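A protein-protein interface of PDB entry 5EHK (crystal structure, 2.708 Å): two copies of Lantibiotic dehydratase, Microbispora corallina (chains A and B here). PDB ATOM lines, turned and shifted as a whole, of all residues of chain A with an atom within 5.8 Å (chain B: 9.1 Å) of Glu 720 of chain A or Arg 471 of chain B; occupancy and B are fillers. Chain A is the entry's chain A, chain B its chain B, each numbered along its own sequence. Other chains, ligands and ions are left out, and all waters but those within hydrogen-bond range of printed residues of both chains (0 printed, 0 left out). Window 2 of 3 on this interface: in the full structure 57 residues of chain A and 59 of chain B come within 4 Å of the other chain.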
ATOM      1  N   ALA A 470      -5.140  14.116 -16.936  1.00  0.00           N
ATOM      2  CA  ALA A 470      -5.583  13.541 -15.661  1.00  0.00           C
ATOM      3  C   ALA A 470      -5.900  12.036 -15.776  1.00  0.00           C
ATOM      4  O   ALA A 470      -5.513  11.253 -14.897  1.00  0.00           O
ATOM      5  CB  ALA A 470      -6.770  14.297 -15.118  1.00  0.00           C
ATOM      6  N   ARG A 471      -6.599  11.653 -16.852  1.00  0.00           N
ATOM      7  CA  ARG A 471      -6.934  10.262 -17.132  1.00  0.00           C
ATOM      8  C   ARG A 471      -5.651   9.433 -17.191  1.00  0.00           C
ATOM      9  O   ARG A 471      -5.540   8.375 -16.571  1.00  0.00           O
ATOM     10  CB  ARG A 471      -7.713  10.140 -18.460  1.00  0.00           C
ATOM     11  CG  ARG A 471      -8.032   8.697 -18.898  1.00  0.00           C
ATOM     12  CD  ARG A 471      -9.055   8.619 -20.049  1.00  0.00           C
ATOM     13  NE  ARG A 471      -8.525   8.035 -21.291  1.00  0.00           N
ATOM     14  CZ  ARG A 471      -7.672   8.641 -22.122  1.00  0.00           C
ATOM     15  NH1 ARG A 471      -7.263   9.880 -21.889  1.00  0.00           N
ATOM     16  NH2 ARG A 471      -7.246   8.021 -23.215  1.00  0.00           N
ATOM     17  N   GLY A 473      -2.787  10.302 -16.054  1.00  0.00           N
ATOM     18  CA  GLY A 473      -1.940  10.558 -14.890  1.00  0.00           C
ATOM     19  C   GLY A 473      -0.620  11.300 -15.099  1.00  0.00           C
ATOM     20  O   GLY A 473       0.240  11.277 -14.225  1.00  0.00           O
ATOM     21  N   GLN A 696      -6.565  21.886   0.692  1.00  0.00           N
ATOM     22  CA  GLN A 696      -6.823  20.785   1.618  1.00  0.00           C
ATOM     23  C   GLN A 696      -5.909  20.817   2.836  1.00  0.00           C
ATOM     24  O   GLN A 696      -6.225  20.244   3.875  1.00  0.00           O
ATOM     25  CB  GLN A 696      -6.591  19.450   0.916  1.00  0.00           C
ATOM     26  CG  GLN A 696      -7.579  19.103  -0.175  1.00  0.00           C
ATOM     27  CD  GLN A 696      -7.173  17.835  -0.890  1.00  0.00           C
ATOM     28  OE1 GLN A 696      -5.992  17.454  -0.877  1.00  0.00           O
ATOM     29  NE2 GLN A 696      -8.139  17.171  -1.520  1.00  0.00           N
ATOM     30  N   ASP A 715       1.328  13.535   3.792  1.00  0.00           N
ATOM     31  CA  ASP A 715       1.534  12.269   3.098  1.00  0.00           C
ATOM     32  C   ASP A 715       0.272  11.871   2.355  1.00  0.00           C
ATOM     33  O   ASP A 715       0.326  11.311   1.251  1.00  0.00           O
ATOM     34  CB  ASP A 715       1.853  11.182   4.123  1.00  0.00           C
ATOM     35  CG  ASP A 715       3.268  11.284   4.668  1.00  0.00           C
ATOM     36  OD1 ASP A 715       4.191  11.658   3.906  1.00  0.00           O
ATOM     37  OD2 ASP A 715       3.448  11.001   5.873  1.00  0.00           O
ATOM     38  N   ARG A 716      -0.865  12.164   2.978  1.00  0.00           N
ATOM     39  CA  ARG A 716      -2.172  11.931   2.377  1.00  0.00           C
ATOM     40  C   ARG A 716      -2.318  12.794   1.127  1.00  0.00           C
ATOM     41  O   ARG A 716      -2.635  12.284   0.054  1.00  0.00           O
ATOM     42  CB  ARG A 716      -3.291  12.163   3.411  1.00  0.00           C
ATOM     43  CG  ARG A 716      -4.689  11.729   2.992  1.00  0.00           C
ATOM     44  CD  ARG A 716      -5.549  11.389   4.218  1.00  0.00           C
ATOM     45  NE  ARG A 716      -5.646  12.486   5.187  1.00  0.00           N
ATOM     46  CZ  ARG A 716      -5.072  12.486   6.391  1.00  0.00           C
ATOM     47  NH1 ARG A 716      -4.345  11.451   6.797  1.00  0.00           N
ATOM     48  NH2 ARG A 716      -5.219  13.526   7.198  1.00  0.00           N
ATOM     49  N   TRP A 717      -2.085  14.099   1.279  1.00  0.00           N
ATOM     50  CA  TRP A 717      -2.073  15.037   0.157  1.00  0.00           C
ATOM     51  C   TRP A 717      -1.015  14.670  -0.873  1.00  0.00           C
ATOM     52  O   TRP A 717      -1.277  14.679  -2.070  1.00  0.00           O
ATOM     53  CB  TRP A 717      -1.836  16.467   0.640  1.00  0.00           C
ATOM     54  CG  TRP A 717      -1.661  17.487  -0.485  1.00  0.00           C
ATOM     55  CD1 TRP A 717      -2.641  18.002  -1.289  1.00  0.00           C
ATOM     56  CD2 TRP A 717      -0.437  18.124  -0.892  1.00  0.00           C
ATOM     57  NE1 TRP A 717      -2.101  18.908  -2.175  1.00  0.00           N
ATOM     58  CE2 TRP A 717      -0.755  19.002  -1.951  1.00  0.00           C
ATOM     59  CE3 TRP A 717       0.891  18.037  -0.464  1.00  0.00           C
ATOM     60  CZ2 TRP A 717       0.208  19.783  -2.584  1.00  0.00           C
ATOM     61  CZ3 TRP A 717       1.843  18.809  -1.093  1.00  0.00           C
ATOM     62  CH2 TRP A 717       1.499  19.674  -2.142  1.00  0.00           C
ATOM     63  N   ARG A 718       0.190  14.379  -0.400  1.00  0.00           N
ATOM     64  CA  ARG A 718       1.299  14.054  -1.284  1.00  0.00           C
ATOM     65  C   ARG A 718       0.993  12.861  -2.182  1.00  0.00           C
ATOM     66  O   ARG A 718       1.296  12.874  -3.373  1.00  0.00           O
ATOM     67  CB  ARG A 718       2.570  13.807  -0.478  1.00  0.00           C
ATOM     68  CG  ARG A 718       3.763  14.563  -1.015  1.00  0.00           C
ATOM     69  CD  ARG A 718       4.867  14.736   0.029  1.00  0.00           C
ATOM     70  NE  ARG A 718       5.625  13.514   0.292  1.00  0.00           N
ATOM     71  CZ  ARG A 718       6.380  12.892  -0.609  1.00  0.00           C
ATOM     72  NH1 ARG A 718       6.457  13.356  -1.849  1.00  0.00           N
ATOM     73  NH2 ARG A 718       7.045  11.792  -0.278  1.00  0.00           N
ATOM     74  N   ALA A 719       0.367  11.837  -1.619  1.00  0.00           N
ATOM     75  CA  ALA A 719       0.094  10.625  -2.380  1.00  0.00           C
ATOM     76  C   ALA A 719      -1.210  10.723  -3.193  1.00  0.00           C
ATOM     77  O   ALA A 719      -1.394  10.002  -4.168  1.00  0.00           O
ATOM     78  CB  ALA A 719       0.062   9.431  -1.454  1.00  0.00           C
ATOM     79  N   GLU A 720      -2.097  11.633  -2.805  1.00  0.00           N
ATOM     80  CA  GLU A 720      -3.389  11.780  -3.463  1.00  0.00           C
ATOM     81  C   GLU A 720      -3.319  12.491  -4.820  1.00  0.00           C
ATOM     82  O   GLU A 720      -4.215  12.326  -5.668  1.00  0.00           O
ATOM     83  CB  GLU A 720      -4.354  12.536  -2.557  1.00  0.00           C
ATOM     84  CG  GLU A 720      -5.754  12.686  -3.136  1.00  0.00           C
ATOM     85  CD  GLU A 720      -6.599  13.607  -2.294  1.00  0.00           C
ATOM     86  OE1 GLU A 720      -6.136  13.924  -1.173  1.00  0.00           O
ATOM     87  OE2 GLU A 720      -7.691  14.034  -2.760  1.00  0.00           O
ATOM     88  N   TRP A 721      -2.285  13.309  -5.021  1.00  0.00           N
ATOM     89  CA  TRP A 721      -2.185  14.089  -6.255  1.00  0.00           C
ATOM     90  C   TRP A 721      -0.853  13.820  -6.940  1.00  0.00           C
ATOM     91  O   TRP A 721      -0.566  14.385  -8.003  1.00  0.00           O
ATOM     92  CB  TRP A 721      -2.350  15.584  -5.966  1.00  0.00           C
ATOM     93  CG  TRP A 721      -3.650  15.915  -5.325  1.00  0.00           C
ATOM     94  CD1 TRP A 721      -3.854  16.276  -4.026  1.00  0.00           C
ATOM     95  CD2 TRP A 721      -4.939  15.887  -5.937  1.00  0.00           C
ATOM     96  NE1 TRP A 721      -5.189  16.491  -3.797  1.00  0.00           N
ATOM     97  CE2 TRP A 721      -5.876  16.250  -4.957  1.00  0.00           C
ATOM     98  CE3 TRP A 721      -5.390  15.591  -7.219  1.00  0.00           C
ATOM     99  CZ2 TRP A 721      -7.234  16.327  -5.222  1.00  0.00           C
ATOM    100  CZ3 TRP A 721      -6.735  15.663  -7.479  1.00  0.00           C
ATOM    101  CH2 TRP A 721      -7.645  16.027  -6.485  1.00  0.00           C
ATOM    102  N   ASN A 722      -0.073  12.920  -6.340  1.00  0.00           N
ATOM    103  CA  ASN A 722       1.234  12.523  -6.849  1.00  0.00           C
ATOM    104  C   ASN A 722       2.248  13.676  -6.806  1.00  0.00           C
ATOM    105  O   ASN A 722       2.966  13.943  -7.769  1.00  0.00           O
ATOM    106  CB  ASN A 722       1.127  11.951  -8.268  1.00  0.00           C
ATOM    107  CG  ASN A 722       2.390  11.210  -8.704  1.00  0.00           C
ATOM    108  OD1 ASN A 722       3.155  10.669  -7.883  1.00  0.00           O
ATOM    109  ND2 ASN A 722       2.643  11.226 -10.008  1.00  0.00           N
ATOM    110  N   ALA B 463     -13.920  22.092  -8.289  1.00  0.00           N
ATOM    111  CA  ALA B 463     -12.846  21.585  -9.137  1.00  0.00           C
ATOM    112  C   ALA B 463     -12.232  20.249  -8.660  1.00  0.00           C
ATOM    113  O   ALA B 463     -12.023  19.336  -9.476  1.00  0.00           O
ATOM    114  CB  ALA B 463     -11.767  22.653  -9.332  1.00  0.00           C
ATOM    115  N   ARG B 464     -11.960  20.124  -7.356  1.00  0.00           N
ATOM    116  CA  ARG B 464     -11.419  18.865  -6.827  1.00  0.00           C
ATOM    117  C   ARG B 464     -12.312  17.694  -7.207  1.00  0.00           C
ATOM    118  O   ARG B 464     -11.830  16.626  -7.593  1.00  0.00           O
ATOM    119  CB  ARG B 464     -11.313  18.891  -5.313  1.00  0.00           C
ATOM    120  CG  ARG B 464     -10.103  19.553  -4.808  1.00  0.00           C
ATOM    121  CD  ARG B 464      -9.875  19.223  -3.338  1.00  0.00           C
ATOM    122  NE  ARG B 464     -11.010  19.559  -2.482  1.00  0.00           N
ATOM    123  CZ  ARG B 464     -11.242  20.780  -2.000  1.00  0.00           C
ATOM    124  NH1 ARG B 464     -10.445  21.791  -2.344  1.00  0.00           N
ATOM    125  NH2 ARG B 464     -12.291  21.001  -1.209  1.00  0.00           N
ATOM    126  N   LEU B 465     -13.617  17.907  -7.079  1.00  0.00           N
ATOM    127  CA  LEU B 465     -14.588  16.873  -7.358  1.00  0.00           C
ATOM    128  C   LEU B 465     -14.438  16.429  -8.795  1.00  0.00           C
ATOM    129  O   LEU B 465     -14.539  15.241  -9.085  1.00  0.00           O
ATOM    130  CB  LEU B 465     -16.015  17.356  -7.077  1.00  0.00           C
ATOM    131  CG  LEU B 465     -16.387  17.708  -5.623  1.00  0.00           C
ATOM    132  CD1 LEU B 465     -17.830  18.180  -5.583  1.00  0.00           C
ATOM    133  CD2 LEU B 465     -16.154  16.552  -4.643  1.00  0.00           C
ATOM    134  N   VAL B 466     -14.193  17.380  -9.691  1.00  0.00           N
ATOM    135  CA  VAL B 466     -14.074  17.055 -11.107  1.00  0.00           C
ATOM    136  C   VAL B 466     -12.759  16.308 -11.337  1.00  0.00           C
ATOM    137  O   VAL B 466     -12.709  15.319 -12.067  1.00  0.00           O
ATOM    138  CB  VAL B 466     -14.170  18.320 -11.993  1.00  0.00           C
ATOM    139  CG1 VAL B 466     -14.031  17.968 -13.466  1.00  0.00           C
ATOM    140  CG2 VAL B 466     -15.498  19.027 -11.749  1.00  0.00           C
ATOM    141  N   ALA B 467     -11.698  16.776 -10.690  1.00  0.00           N
ATOM    142  CA  ALA B 467     -10.386  16.174 -10.870  1.00  0.00           C
ATOM    143  C   ALA B 467     -10.360  14.750 -10.318  1.00  0.00           C
ATOM    144  O   ALA B 467     -10.029  13.816 -11.048  1.00  0.00           O
ATOM    145  CB  ALA B 467      -9.323  17.012 -10.210  1.00  0.00           C
ATOM    146  N   LYS B 468     -10.721  14.593  -9.042  1.00  0.00           N
ATOM    147  CA  LYS B 468     -10.824  13.276  -8.419  1.00  0.00           C
ATOM    148  C   LYS B 468     -11.631  12.323  -9.283  1.00  0.00           C
ATOM    149  O   LYS B 468     -11.189  11.208  -9.569  1.00  0.00           O
ATOM    150  CB  LYS B 468     -11.407  13.373  -7.015  1.00  0.00           C
ATOM    151  CG  LYS B 468     -10.414  13.935  -6.004  1.00  0.00           C
ATOM    152  CD  LYS B 468     -10.981  14.017  -4.589  1.00  0.00           C
ATOM    153  CE  LYS B 468     -12.115  15.053  -4.477  1.00  0.00           C
ATOM    154  NZ  LYS B 468     -12.711  15.163  -3.098  1.00  0.00           N
ATOM    155  N   ALA B 469     -12.804  12.761  -9.715  1.00  0.00           N
ATOM    156  CA  ALA B 469     -13.598  11.959 -10.627  1.00  0.00           C
ATOM    157  C   ALA B 469     -12.841  11.600 -11.902  1.00  0.00           C
ATOM    158  O   ALA B 469     -13.073  10.545 -12.475  1.00  0.00           O
ATOM    159  CB  ALA B 469     -14.880  12.679 -10.984  1.00  0.00           C
ATOM    160  N   ALA B 470     -11.924  12.456 -12.340  1.00  0.00           N
ATOM    161  CA  ALA B 470     -11.224  12.212 -13.607  1.00  0.00           C
ATOM    162  C   ALA B 470     -10.074  11.211 -13.474  1.00  0.00           C
ATOM    163  O   ALA B 470      -9.883  10.340 -14.328  1.00  0.00           O
ATOM    164  CB  ALA B 470     -10.708  13.513 -14.186  1.00  0.00           C
ATOM    165  N   ARG B 471      -9.298  11.373 -12.412  1.00  0.00           N
ATOM    166  CA  ARG B 471      -8.181  10.502 -12.147  1.00  0.00           C
ATOM    167  C   ARG B 471      -8.701   9.078 -12.091  1.00  0.00           C
ATOM    168  O   ARG B 471      -8.162   8.175 -12.726  1.00  0.00           O
ATOM    169  CB  ARG B 471      -7.543  10.884 -10.814  1.00  0.00           C
ATOM    170  CG  ARG B 471      -6.925  12.255 -10.816  1.00  0.00           C
ATOM    171  CD  ARG B 471      -5.576  12.271 -11.536  1.00  0.00           C
ATOM    172  NE  ARG B 471      -4.682  11.234 -11.027  1.00  0.00           N
ATOM    173  CZ  ARG B 471      -4.105  11.256  -9.826  1.00  0.00           C
ATOM    174  NH1 ARG B 471      -4.318  12.274  -8.993  1.00  0.00           N
ATOM    175  NH2 ARG B 471      -3.314  10.254  -9.454  1.00  0.00           N
ATOM    176  N   ARG B 472      -9.781   8.897 -11.350  1.00  0.00           N
ATOM    177  CA  ARG B 472     -10.320   7.572 -11.111  1.00  0.00           C
ATOM    178  C   ARG B 472     -11.431   7.161 -12.090  1.00  0.00           C
ATOM    179  O   ARG B 472     -12.123   6.183 -11.863  1.00  0.00           O
ATOM    180  CB  ARG B 472     -10.651   7.388  -9.621  1.00  0.00           C
ATOM    181  CG  ARG B 472      -9.357   7.431  -8.774  1.00  0.00           C
ATOM    182  CD  ARG B 472      -9.566   7.557  -7.280  1.00  0.00           C
ATOM    183  NE  ARG B 472     -10.886   8.077  -6.900  1.00  0.00           N
ATOM    184  CZ  ARG B 472     -11.744   7.466  -6.074  1.00  0.00           C
ATOM    185  NH1 ARG B 472     -11.437   6.290  -5.535  1.00  0.00           N
ATOM    186  NH2 ARG B 472     -12.914   8.029  -5.788  1.00  0.00           N
ATOM    187  N   GLY B 473     -11.602   7.933 -13.164  1.00  0.00           N
ATOM    188  CA  GLY B 473     -12.477   7.569 -14.274  1.00  0.00           C
ATOM    189  C   GLY B 473     -13.958   7.404 -13.980  1.00  0.00           C
ATOM    190  O   GLY B 473     -14.705   6.859 -14.788  1.00  0.00           O
ATOM    191  N   GLU B 474     -14.389   7.934 -12.842  1.00  0.00           N
ATOM    192  CA  GLU B 474     -15.757   7.783 -12.345  1.00  0.00           C
ATOM    193  C   GLU B 474     -16.765   8.731 -13.028  1.00  0.00           C
ATOM    194  O   GLU B 474     -16.464   9.890 -13.298  1.00  0.00           O
ATOM    195  CB  GLU B 474     -15.740   7.995 -10.822  1.00  0.00           C
ATOM    196  CG  GLU B 474     -14.902   6.960 -10.054  1.00  0.00           C
ATOM    197  CD  GLU B 474     -14.533   7.409  -8.630  1.00  0.00           C
ATOM    198  OE1 GLU B 474     -14.499   8.633  -8.361  1.00  0.00           O
ATOM    199  OE2 GLU B 474     -14.277   6.543  -7.766  1.00  0.00           O
ATOM    200  N   ILE B 477     -19.805  11.615  -8.856  1.00  0.00           N
ATOM    201  CA  ILE B 477     -19.112  11.925  -7.628  1.00  0.00           C
ATOM    202  C   ILE B 477     -20.204  11.985  -6.574  1.00  0.00           C
ATOM    203  O   ILE B 477     -21.334  12.379  -6.856  1.00  0.00           O
ATOM    204  CB  ILE B 477     -18.276  13.230  -7.717  1.00  0.00           C
ATOM    205  CG1 ILE B 477     -17.199  13.266  -6.618  1.00  0.00           C
ATOM    206  CG2 ILE B 477     -19.161  14.453  -7.700  1.00  0.00           C
ATOM    207  CD1 ILE B 477     -15.870  12.487  -6.967  1.00  0.00           C
ATOM    208  N   PHE B 676     -15.914  16.590 -19.877  1.00  0.00           N
ATOM    209  CA  PHE B 676     -16.830  15.753 -19.156  1.00  0.00           C
ATOM    210  C   PHE B 676     -17.094  16.295 -17.757  1.00  0.00           C
ATOM    211  O   PHE B 676     -16.170  16.661 -17.030  1.00  0.00           O
ATOM    212  CB  PHE B 676     -16.351  14.288 -19.108  1.00  0.00           C
ATOM    213  CG  PHE B 676     -17.177  13.433 -18.201  1.00  0.00           C
ATOM    214  CD1 PHE B 676     -18.443  13.010 -18.599  1.00  0.00           C
ATOM    215  CD2 PHE B 676     -16.721  13.113 -16.926  1.00  0.00           C
ATOM    216  CE1 PHE B 676     -19.223  12.258 -17.763  1.00  0.00           C
ATOM    217  CE2 PHE B 676     -17.492  12.356 -16.076  1.00  0.00           C
ATOM    218  CZ  PHE B 676     -18.751  11.925 -16.494  1.00  0.00           C
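Of the 12 printed residues of chain A, 4 touch a printed residue of chain B. Printed residues of chain A that touch a printed residue of chain B: Ala 470, Gln 696, Glu 720 and Trp 721. Of the 14 printed residues of chain B, 4 touch a printed residue of chain A. Hydrophobic or aromatic side chains of chain B within 4 Å of the printed part of chain A: Ala 467. Among the printed residues, 7 pairs touch across the chains. Among the printed residues, no Asp or Glu carboxylate lies within 4 Å of a Lys or Arg side-chain nitrogen of the other chain.
Ala 470 of chain A touches Arg 471 of chain B, but with the chains exchanged Arg 471 of chain A does not touch Ala 470 of chain B (4.1 Å).
Ala 470 of chain A touches Arg 471 of chain B (O to CD, 3.5 Å). Gln 696 of chain A touches Arg 464 of chain B (NE2 to CD, 3.2 Å). Glu 720 of chain A touches Lys 468 of chain B (OE2 to CD, 3.8 Å). Trp 721 of chain A touches Ala 467 of chain B. Lys 468 of chain B touches Trp 721 of chain A (CG to CH2, 3.5 Å). Arg 471 of chain B touches Trp 721 of chain A (NH1 to CE3, 3.9 Å).
Glu 720 of chain A touches just these residues of chain B: Lys 468 (3.8 Å) and Arg 471 (3.3 Å). Printed residues of chain A within 4 Å of Arg 471 of chain B: Ala 470, Glu 720 and Trp 721. Ala 719 of chain A touches none of the printed residues of chain B. Of the printed residues of chain A, Ala 467 of chain B touches Trp 721 (3.997 Å). Of the printed residues of chain B, Trp 721 of chain A touches Ala 467, Lys 468 and Arg 471. The nearest residue of chain A that does not touch Arg 471 of chain B is Arg 471 of chain A (4.7 Å).
NH1 of Arg 471 of chain B sits at hydrogen-bond distance from O of Glu 720 of chain A (3.3 Å).
NE1 of Trp 721 of chain A lies within hydrogen-bond range of OE1 of Gln 696 of chain A, 3.2 Å away. NE2 of Gln 696 of chain A sits at hydrogen-bond distance from OE2 of Glu 720 of chain A, 3.4 Å away.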
